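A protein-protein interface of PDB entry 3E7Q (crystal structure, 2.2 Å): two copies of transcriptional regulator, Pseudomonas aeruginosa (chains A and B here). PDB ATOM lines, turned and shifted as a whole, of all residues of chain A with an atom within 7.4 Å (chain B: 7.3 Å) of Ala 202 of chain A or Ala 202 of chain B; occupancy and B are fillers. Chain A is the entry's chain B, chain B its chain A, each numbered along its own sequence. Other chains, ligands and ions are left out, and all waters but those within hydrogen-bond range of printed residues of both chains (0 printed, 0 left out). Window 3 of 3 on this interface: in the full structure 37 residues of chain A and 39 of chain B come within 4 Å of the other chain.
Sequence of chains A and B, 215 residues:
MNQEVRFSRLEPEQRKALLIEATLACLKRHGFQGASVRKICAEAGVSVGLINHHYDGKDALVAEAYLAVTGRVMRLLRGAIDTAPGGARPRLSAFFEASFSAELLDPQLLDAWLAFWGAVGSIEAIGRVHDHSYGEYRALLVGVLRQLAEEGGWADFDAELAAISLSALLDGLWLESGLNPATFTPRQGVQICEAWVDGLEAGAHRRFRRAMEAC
Gly 199 of chain A touches its own counterpart, Gly 199 of chain B.
Gly 199 of chain A touches Ala 204 of chain B, and with the chains exchanged Ala 204 of chain A touches Gly 199 of chain B.
Ala 202 of chain B touches its own counterpart, Ala 202 of chain A.
Positions printed for both chains: 89, 154, 196, 197, 198, 199, 200, 201, 202, 203, 204, 205 and 206.
Of the 4 pairs that touch across the chains among the printed residues, 4 have their exchanged pair printed and touching as well.
Ala 202 of chain A touches just one residue of chain B: Ala 202.
Of chain A, only Ala 202 comes within 4 Å of Ala 202 of chain B.
Of the printed residues of chain A, Ala 204 of chain B touches Gly 199.
Printed residues of chain B within 4 Å of Gly 199 of chain A: Gly 199 and Ala 204.
Printed residues of chain B within 4 Å of Ala 204 of chain A: Gly 199.
Of the printed residues of chain A, Gly 199 of chain B touches Gly 199 and Ala 204.
Glu 201 of chain B touches none of the printed residues of chain A.
Arg 89 of chain A touches none of the printed residues of chain B.
The nearest residue of chain A that does not touch Ala 202 of chain B is Gly 203 of chain A (4.2 Å).
The nearest printed residue of chain B that does not touch Ala 204 of chain A is Asp 198 of chain B (4.2 Å).
The backbone NH of Ala 204 of chain A lies within hydrogen-bond range of the backbone carbonyl oxygen of Gly 199 of chain A.
The backbone NH (N) of Ala 204 of chain B sits close to the backbone carbonyl oxygen (O) of Gly 199 of chain B.
Printed residues of chain B that touch a printed residue of chain A: Gly 199, Ala 202 and Ala 204.
Printed residues of chain A that touch a printed residue of chain B: Gly 199, Ala 202 and Ala 204.
Hydrophobic or aromatic side chains of chain A within 4 Å of the printed part of chain B: Ala 202 and Ala 204.
Among the printed residues, 4 pairs touch across the chains.
O of Gly 199 of chain B touches CA of Gly 199 of chain A, 3.5 Å away.
Ala 204 of chain B touches Gly 199 of chain A.
Ala 202 of chain A touches Ala 202 of chain B.
Gly 199 of chain B touches Ala 204 of chain A.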
ATOM      1  N   ARG A  89     -41.870   1.893  10.572  1.00  0.00           N
ATOM      2  CA  ARG A  89     -40.729   2.647  10.017  1.00  0.00           C
ATOM      3  C   ARG A  89     -41.181   3.716   9.025  1.00  0.00           C
ATOM      4  O   ARG A  89     -40.696   4.846   9.081  1.00  0.00           O
ATOM      5  CB  ARG A  89     -39.633   1.721   9.440  1.00  0.00           C
ATOM      6  CG  ARG A  89     -38.935   0.979  10.557  1.00  0.00           C
ATOM      7  CD  ARG A  89     -37.420   0.930  10.577  1.00  0.00           C
ATOM      8  NE  ARG A  89     -36.670   2.188  10.334  1.00  0.00           N
ATOM      9  CZ  ARG A  89     -35.340   2.255  10.377  1.00  0.00           C
ATOM     10  NH1 ARG A  89     -34.652   1.202  10.735  1.00  0.00           N
ATOM     11  NH2 ARG A  89     -34.706   3.369  10.107  1.00  0.00           N
ATOM     12  N   TRP A 154     -39.996  -7.580  19.991  1.00  0.00           N
ATOM     13  CA  TRP A 154     -39.101  -7.384  21.127  1.00  0.00           C
ATOM     14  C   TRP A 154     -39.833  -7.718  22.412  1.00  0.00           C
ATOM     15  O   TRP A 154     -40.919  -7.229  22.666  1.00  0.00           O
ATOM     16  CB  TRP A 154     -38.591  -5.952  21.099  1.00  0.00           C
ATOM     17  CG  TRP A 154     -37.969  -5.590  19.719  1.00  0.00           C
ATOM     18  CD1 TRP A 154     -37.458  -6.448  18.814  1.00  0.00           C
ATOM     19  CD2 TRP A 154     -37.741  -4.284  19.194  1.00  0.00           C
ATOM     20  NE1 TRP A 154     -36.951  -5.781  17.731  1.00  0.00           N
ATOM     21  CE2 TRP A 154     -37.136  -4.442  17.927  1.00  0.00           C
ATOM     22  CE3 TRP A 154     -38.010  -2.987  19.655  1.00  0.00           C
ATOM     23  CZ2 TRP A 154     -36.812  -3.366  17.124  1.00  0.00           C
ATOM     24  CZ3 TRP A 154     -37.668  -1.905  18.844  1.00  0.00           C
ATOM     25  CH2 TRP A 154     -37.080  -2.100  17.607  1.00  0.00           C
ATOM     26  N   TRP A 196     -30.642   6.227  14.344  1.00  0.00           N
ATOM     27  CA  TRP A 196     -31.042   5.864  15.682  1.00  0.00           C
ATOM     28  C   TRP A 196     -31.999   4.649  15.728  1.00  0.00           C
ATOM     29  O   TRP A 196     -31.870   3.752  16.556  1.00  0.00           O
ATOM     30  CB  TRP A 196     -31.777   7.065  16.297  1.00  0.00           C
ATOM     31  CG  TRP A 196     -32.192   6.860  17.685  1.00  0.00           C
ATOM     32  CD1 TRP A 196     -31.459   7.169  18.760  1.00  0.00           C
ATOM     33  CD2 TRP A 196     -33.454   6.326  18.192  1.00  0.00           C
ATOM     34  NE1 TRP A 196     -32.156   6.878  19.902  1.00  0.00           N
ATOM     35  CE2 TRP A 196     -33.366   6.340  19.593  1.00  0.00           C
ATOM     36  CE3 TRP A 196     -34.614   5.837  17.604  1.00  0.00           C
ATOM     37  CZ2 TRP A 196     -34.384   5.874  20.430  1.00  0.00           C
ATOM     38  CZ3 TRP A 196     -35.638   5.376  18.436  1.00  0.00           C
ATOM     39  CH2 TRP A 196     -35.517   5.419  19.842  1.00  0.00           C
ATOM     40  N   VAL A 197     -33.028   4.715  14.902  1.00  0.00           N
ATOM     41  CA  VAL A 197     -33.961   3.581  14.739  1.00  0.00           C
ATOM     42  C   VAL A 197     -33.240   2.340  14.292  1.00  0.00           C
ATOM     43  O   VAL A 197     -33.522   1.266  14.815  1.00  0.00           O
ATOM     44  CB  VAL A 197     -35.150   3.893  13.759  1.00  0.00           C
ATOM     45  CG1 VAL A 197     -36.167   2.806  13.784  1.00  0.00           C
ATOM     46  CG2 VAL A 197     -35.807   5.258  14.123  1.00  0.00           C
ATOM     47  N   ASP A 198     -32.309   2.497  13.337  1.00  0.00           N
ATOM     48  CA  ASP A 198     -31.473   1.381  12.882  1.00  0.00           C
ATOM     49  C   ASP A 198     -30.772   0.748  14.065  1.00  0.00           C
ATOM     50  O   ASP A 198     -30.726  -0.473  14.192  1.00  0.00           O
ATOM     51  CB  ASP A 198     -30.357   1.811  11.913  1.00  0.00           C
ATOM     52  CG  ASP A 198     -30.846   2.213  10.534  1.00  0.00           C
ATOM     53  OD1 ASP A 198     -32.019   2.036  10.175  1.00  0.00           O
ATOM     54  OD2 ASP A 198     -29.996   2.726   9.784  1.00  0.00           O
ATOM     55  N   GLY A 199     -30.168   1.596  14.889  1.00  0.00           N
ATOM     56  CA  GLY A 199     -29.507   1.175  16.122  1.00  0.00           C
ATOM     57  C   GLY A 199     -30.354   0.317  17.042  1.00  0.00           C
ATOM     58  O   GLY A 199     -29.936  -0.751  17.433  1.00  0.00           O
ATOM     59  N   LEU A 200     -31.527   0.805  17.400  1.00  0.00           N
ATOM     60  CA  LEU A 200     -32.539  -0.029  18.056  1.00  0.00           C
ATOM     61  C   LEU A 200     -32.770  -1.355  17.401  1.00  0.00           C
ATOM     62  O   LEU A 200     -32.638  -2.364  18.005  1.00  0.00           O
ATOM     63  CB  LEU A 200     -33.886   0.656  18.044  1.00  0.00           C
ATOM     64  CG  LEU A 200     -34.338   1.580  19.139  1.00  0.00           C
ATOM     65  CD1 LEU A 200     -35.859   1.774  18.918  1.00  0.00           C
ATOM     66  CD2 LEU A 200     -34.091   1.086  20.514  1.00  0.00           C
ATOM     67  N   GLU A 201     -33.112  -1.332  16.124  1.00  0.00           N
ATOM     68  CA  GLU A 201     -33.413  -2.559  15.410  1.00  0.00           C
ATOM     69  C   GLU A 201     -32.242  -3.546  15.342  1.00  0.00           C
ATOM     70  O   GLU A 201     -32.476  -4.767  15.304  1.00  0.00           O
ATOM     71  CB  GLU A 201     -33.917  -2.247  14.005  1.00  0.00           C
ATOM     72  CG  GLU A 201     -35.239  -1.547  13.968  1.00  0.00           C
ATOM     73  CD  GLU A 201     -36.103  -2.089  12.867  1.00  0.00           C
ATOM     74  OE1 GLU A 201     -36.089  -1.547  11.726  1.00  0.00           O
ATOM     75  OE2 GLU A 201     -36.764  -3.126  13.134  1.00  0.00           O
ATOM     76  N   ALA A 202     -31.010  -3.015  15.350  1.00  0.00           N
ATOM     77  CA  ALA A 202     -29.802  -3.830  15.262  1.00  0.00           C
ATOM     78  C   ALA A 202     -29.520  -4.537  16.577  1.00  0.00           C
ATOM     79  O   ALA A 202     -28.831  -5.532  16.585  1.00  0.00           O
ATOM     80  CB  ALA A 202     -28.595  -3.020  14.799  1.00  0.00           C
ATOM     81  N   GLY A 203     -30.088  -4.052  17.672  1.00  0.00           N
ATOM     82  CA  GLY A 203     -30.053  -4.765  18.958  1.00  0.00           C
ATOM     83  C   GLY A 203     -30.057  -3.861  20.186  1.00  0.00           C
ATOM     84  O   GLY A 203     -30.225  -4.336  21.294  1.00  0.00           O
ATOM     85  N   ALA A 204     -29.935  -2.549  19.975  1.00  0.00           N
ATOM     86  CA  ALA A 204     -29.968  -1.591  21.039  1.00  0.00           C
ATOM     87  C   ALA A 204     -31.273  -1.539  21.848  1.00  0.00           C
ATOM     88  O   ALA A 204     -31.281  -0.985  22.956  1.00  0.00           O
ATOM     89  CB  ALA A 204     -29.615  -0.185  20.487  1.00  0.00           C
ATOM     90  N   HIS A 205     -32.350  -2.091  21.280  1.00  0.00           N
ATOM     91  CA  HIS A 205     -33.629  -2.229  21.955  1.00  0.00           C
ATOM     92  C   HIS A 205     -33.479  -3.073  23.248  1.00  0.00           C
ATOM     93  O   HIS A 205     -34.246  -2.888  24.186  1.00  0.00           O
ATOM     94  CB  HIS A 205     -34.681  -2.865  21.009  1.00  0.00           C
ATOM     95  CG  HIS A 205     -34.444  -4.318  20.712  1.00  0.00           C
ATOM     96  ND1 HIS A 205     -34.793  -5.323  21.584  1.00  0.00           N
ATOM     97  CD2 HIS A 205     -33.901  -4.934  19.641  1.00  0.00           C
ATOM     98  CE1 HIS A 205     -34.461  -6.492  21.077  1.00  0.00           C
ATOM     99  NE2 HIS A 205     -33.917  -6.283  19.897  1.00  0.00           N
ATOM    100  N   ARG A 206     -32.477  -3.969  23.283  1.00  0.00           N
ATOM    101  CA  ARG A 206     -32.116  -4.723  24.486  1.00  0.00           C
ATOM    102  C   ARG A 206     -31.649  -3.898  25.701  1.00  0.00           C
ATOM    103  O   ARG A 206     -31.902  -4.282  26.860  1.00  0.00           O
ATOM    104  CB  ARG A 206     -31.092  -5.797  24.143  1.00  0.00           C
ATOM    105  CG  ARG A 206     -31.735  -6.898  23.295  1.00  0.00           C
ATOM    106  CD  ARG A 206     -30.810  -8.050  22.984  1.00  0.00           C
ATOM    107  NE  ARG A 206     -29.488  -7.580  22.563  1.00  0.00           N
ATOM    108  CZ  ARG A 206     -29.026  -7.596  21.308  1.00  0.00           C
ATOM    109  NH1 ARG A 206     -29.777  -8.075  20.305  1.00  0.00           N
ATOM    110  NH2 ARG A 206     -27.788  -7.135  21.044  1.00  0.00           N
ATOM    111  N   ARG B  89     -15.169   3.047  25.132  1.00  0.00           N
ATOM    112  CA  ARG B  89     -16.445   2.950  25.873  1.00  0.00           C
ATOM    113  C   ARG B  89     -16.364   3.342  27.355  1.00  0.00           C
ATOM    114  O   ARG B  89     -17.257   4.034  27.845  1.00  0.00           O
ATOM    115  CB  ARG B  89     -17.102   1.570  25.703  1.00  0.00           C
ATOM    116  CG  ARG B  89     -17.523   1.339  24.260  1.00  0.00           C
ATOM    117  CD  ARG B  89     -18.836   0.665  24.105  1.00  0.00           C
ATOM    118  NE  ARG B  89     -19.953   1.266  24.853  1.00  0.00           N
ATOM    119  CZ  ARG B  89     -21.213   0.881  24.693  1.00  0.00           C
ATOM    120  NH1 ARG B  89     -21.521  -0.036  23.793  1.00  0.00           N
ATOM    121  NH2 ARG B  89     -22.176   1.445  25.384  1.00  0.00           N
ATOM    122  N   TRP B 154     -14.560   0.272  12.000  1.00  0.00           N
ATOM    123  CA  TRP B 154     -15.529   0.703  11.030  1.00  0.00           C
ATOM    124  C   TRP B 154     -14.836   1.424   9.885  1.00  0.00           C
ATOM    125  O   TRP B 154     -14.047   2.357  10.094  1.00  0.00           O
ATOM    126  CB  TRP B 154     -16.575   1.578  11.702  1.00  0.00           C
ATOM    127  CG  TRP B 154     -17.166   0.917  12.916  1.00  0.00           C
ATOM    128  CD1 TRP B 154     -17.318  -0.439  13.133  1.00  0.00           C
ATOM    129  CD2 TRP B 154     -17.709   1.570  14.072  1.00  0.00           C
ATOM    130  NE1 TRP B 154     -17.914  -0.656  14.356  1.00  0.00           N
ATOM    131  CE2 TRP B 154     -18.158   0.561  14.952  1.00  0.00           C
ATOM    132  CE3 TRP B 154     -17.845   2.915  14.456  1.00  0.00           C
ATOM    133  CZ2 TRP B 154     -18.744   0.852  16.181  1.00  0.00           C
ATOM    134  CZ3 TRP B 154     -18.448   3.200  15.688  1.00  0.00           C
ATOM    135  CH2 TRP B 154     -18.876   2.175  16.529  1.00  0.00           C
ATOM    136  N   TRP B 196     -27.556   4.359  22.896  1.00  0.00           N
ATOM    137  CA  TRP B 196     -27.171   4.980  21.651  1.00  0.00           C
ATOM    138  C   TRP B 196     -25.831   4.441  21.114  1.00  0.00           C
ATOM    139  O   TRP B 196     -25.652   4.278  19.895  1.00  0.00           O
ATOM    140  CB  TRP B 196     -27.063   6.479  21.867  1.00  0.00           C
ATOM    141  CG  TRP B 196     -26.716   7.285  20.657  1.00  0.00           C
ATOM    142  CD1 TRP B 196     -27.591   7.954  19.870  1.00  0.00           C
ATOM    143  CD2 TRP B 196     -25.412   7.536  20.109  1.00  0.00           C
ATOM    144  NE1 TRP B 196     -26.927   8.614  18.889  1.00  0.00           N
ATOM    145  CE2 TRP B 196     -25.587   8.347  18.993  1.00  0.00           C
ATOM    146  CE3 TRP B 196     -24.132   7.131  20.438  1.00  0.00           C
ATOM    147  CZ2 TRP B 196     -24.516   8.786  18.203  1.00  0.00           C
ATOM    148  CZ3 TRP B 196     -23.078   7.559  19.666  1.00  0.00           C
ATOM    149  CH2 TRP B 196     -23.278   8.400  18.569  1.00  0.00           C
ATOM    150  N   VAL B 197     -24.862   4.289  22.010  1.00  0.00           N
ATOM    151  CA  VAL B 197     -23.537   3.734  21.640  1.00  0.00           C
ATOM    152  C   VAL B 197     -23.695   2.247  21.268  1.00  0.00           C
ATOM    153  O   VAL B 197     -23.175   1.841  20.265  1.00  0.00           O
ATOM    154  CB  VAL B 197     -22.409   3.987  22.777  1.00  0.00           C
ATOM    155  CG1 VAL B 197     -21.046   3.483  22.328  1.00  0.00           C
ATOM    156  CG2 VAL B 197     -22.281   5.456  23.079  1.00  0.00           C
ATOM    157  N   ASP B 198     -24.448   1.450  22.045  1.00  0.00           N
ATOM    158  CA  ASP B 198     -24.813   0.057  21.639  1.00  0.00           C
ATOM    159  C   ASP B 198     -25.351  -0.009  20.256  1.00  0.00           C
ATOM    160  O   ASP B 198     -25.033  -0.926  19.499  1.00  0.00           O
ATOM    161  CB  ASP B 198     -25.934  -0.519  22.500  1.00  0.00           C
ATOM    162  CG  ASP B 198     -25.516  -0.797  23.957  1.00  0.00           C
ATOM    163  OD1 ASP B 198     -24.357  -0.518  24.340  1.00  0.00           O
ATOM    164  OD2 ASP B 198     -26.353  -1.319  24.719  1.00  0.00           O
ATOM    165  N   GLY B 199     -26.245   0.927  19.937  1.00  0.00           N
ATOM    166  CA  GLY B 199     -26.879   1.015  18.647  1.00  0.00           C
ATOM    167  C   GLY B 199     -25.905   1.156  17.504  1.00  0.00           C
ATOM    168  O   GLY B 199     -26.062   0.483  16.485  1.00  0.00           O
ATOM    169  N   LEU B 200     -24.873   1.997  17.701  1.00  0.00           N
ATOM    170  CA  LEU B 200     -23.782   2.107  16.745  1.00  0.00           C
ATOM    171  C   LEU B 200     -22.963   0.834  16.597  1.00  0.00           C
ATOM    172  O   LEU B 200     -22.617   0.431  15.480  1.00  0.00           O
ATOM    173  CB  LEU B 200     -22.806   3.195  17.139  1.00  0.00           C
ATOM    174  CG  LEU B 200     -22.900   4.675  16.800  1.00  0.00           C
ATOM    175  CD1 LEU B 200     -21.473   5.083  17.102  1.00  0.00           C
ATOM    176  CD2 LEU B 200     -23.190   5.091  15.391  1.00  0.00           C
ATOM    177  N   GLU B 201     -22.599   0.230  17.716  1.00  0.00           N
ATOM    178  CA  GLU B 201     -21.767  -0.962  17.676  1.00  0.00           C
ATOM    179  C   GLU B 201     -22.532  -2.138  17.075  1.00  0.00           C
ATOM    180  O   GLU B 201     -21.968  -3.074  16.563  1.00  0.00           O
ATOM    181  CB  GLU B 201     -21.343  -1.368  19.076  1.00  0.00           C
ATOM    182  CG  GLU B 201     -20.284  -0.525  19.689  1.00  0.00           C
ATOM    183  CD  GLU B 201     -19.472  -1.297  20.656  1.00  0.00           C
ATOM    184  OE1 GLU B 201     -19.239  -0.799  21.756  1.00  0.00           O
ATOM    185  OE2 GLU B 201     -19.076  -2.438  20.307  1.00  0.00           O
ATOM    186  N   ALA B 202     -23.831  -2.116  17.220  1.00  0.00           N
ATOM    187  CA  ALA B 202     -24.645  -3.160  16.663  1.00  0.00           C
ATOM    188  C   ALA B 202     -24.785  -3.008  15.135  1.00  0.00           C
ATOM    189  O   ALA B 202     -25.227  -3.921  14.511  1.00  0.00           O
ATOM    190  CB  ALA B 202     -26.015  -3.212  17.367  1.00  0.00           C
ATOM    191  N   GLY B 203     -24.440  -1.865  14.541  1.00  0.00           N
ATOM    192  CA  GLY B 203     -24.435  -1.749  13.096  1.00  0.00           C
ATOM    193  C   GLY B 203     -24.842  -0.421  12.531  1.00  0.00           C
ATOM    194  O   GLY B 203     -24.616  -0.151  11.360  1.00  0.00           O
ATOM    195  N   ALA B 204     -25.475   0.399  13.348  1.00  0.00           N
ATOM    196  CA  ALA B 204     -25.797   1.744  12.982  1.00  0.00           C
ATOM    197  C   ALA B 204     -24.587   2.553  12.552  1.00  0.00           C
ATOM    198  O   ALA B 204     -24.748   3.543  11.862  1.00  0.00           O
ATOM    199  CB  ALA B 204     -26.448   2.414  14.097  1.00  0.00           C
ATOM    200  N   HIS B 205     -23.383   2.159  12.937  1.00  0.00           N
ATOM    201  CA  HIS B 205     -22.193   2.836  12.400  1.00  0.00           C
ATOM    202  C   HIS B 205     -22.243   2.969  10.859  1.00  0.00           C
ATOM    203  O   HIS B 205     -21.694   3.931  10.312  1.00  0.00           O
ATOM    204  CB  HIS B 205     -20.907   2.155  12.869  1.00  0.00           C
ATOM    205  CG  HIS B 205     -20.748   0.733  12.407  1.00  0.00           C
ATOM    206  ND1 HIS B 205     -20.196   0.404  11.184  1.00  0.00           N
ATOM    207  CD2 HIS B 205     -21.040  -0.445  13.015  1.00  0.00           C
ATOM    208  CE1 HIS B 205     -20.180  -0.913  11.053  1.00  0.00           C
ATOM    209  NE2 HIS B 205     -20.680  -1.451  12.153  1.00  0.00           N
ATOM    210  N   ARG B 206     -22.934   2.014  10.196  1.00  0.00           N
ATOM    211  CA  ARG B 206     -23.053   1.922   8.725  1.00  0.00           C
ATOM    212  C   ARG B 206     -23.796   3.081   8.118  1.00  0.00           C
ATOM    213  O   ARG B 206     -23.464   3.525   7.033  1.00  0.00           O
ATOM    214  CB  ARG B 206     -23.815   0.659   8.317  1.00  0.00           C
ATOM    215  CG  ARG B 206     -23.016  -0.578   8.327  1.00  0.00           C
ATOM    216  CD  ARG B 206     -23.755  -1.682   7.555  1.00  0.00           C
ATOM    217  NE  ARG B 206     -24.884  -2.200   8.327  1.00  0.00           N
ATOM    218  CZ  ARG B 206     -24.771  -3.051   9.349  1.00  0.00           C
ATOM    219  NH1 ARG B 206     -23.571  -3.501   9.718  1.00  0.00           N
ATOM    220  NH2 ARG B 206     -25.864  -3.448  10.007  1.00  0.00           N
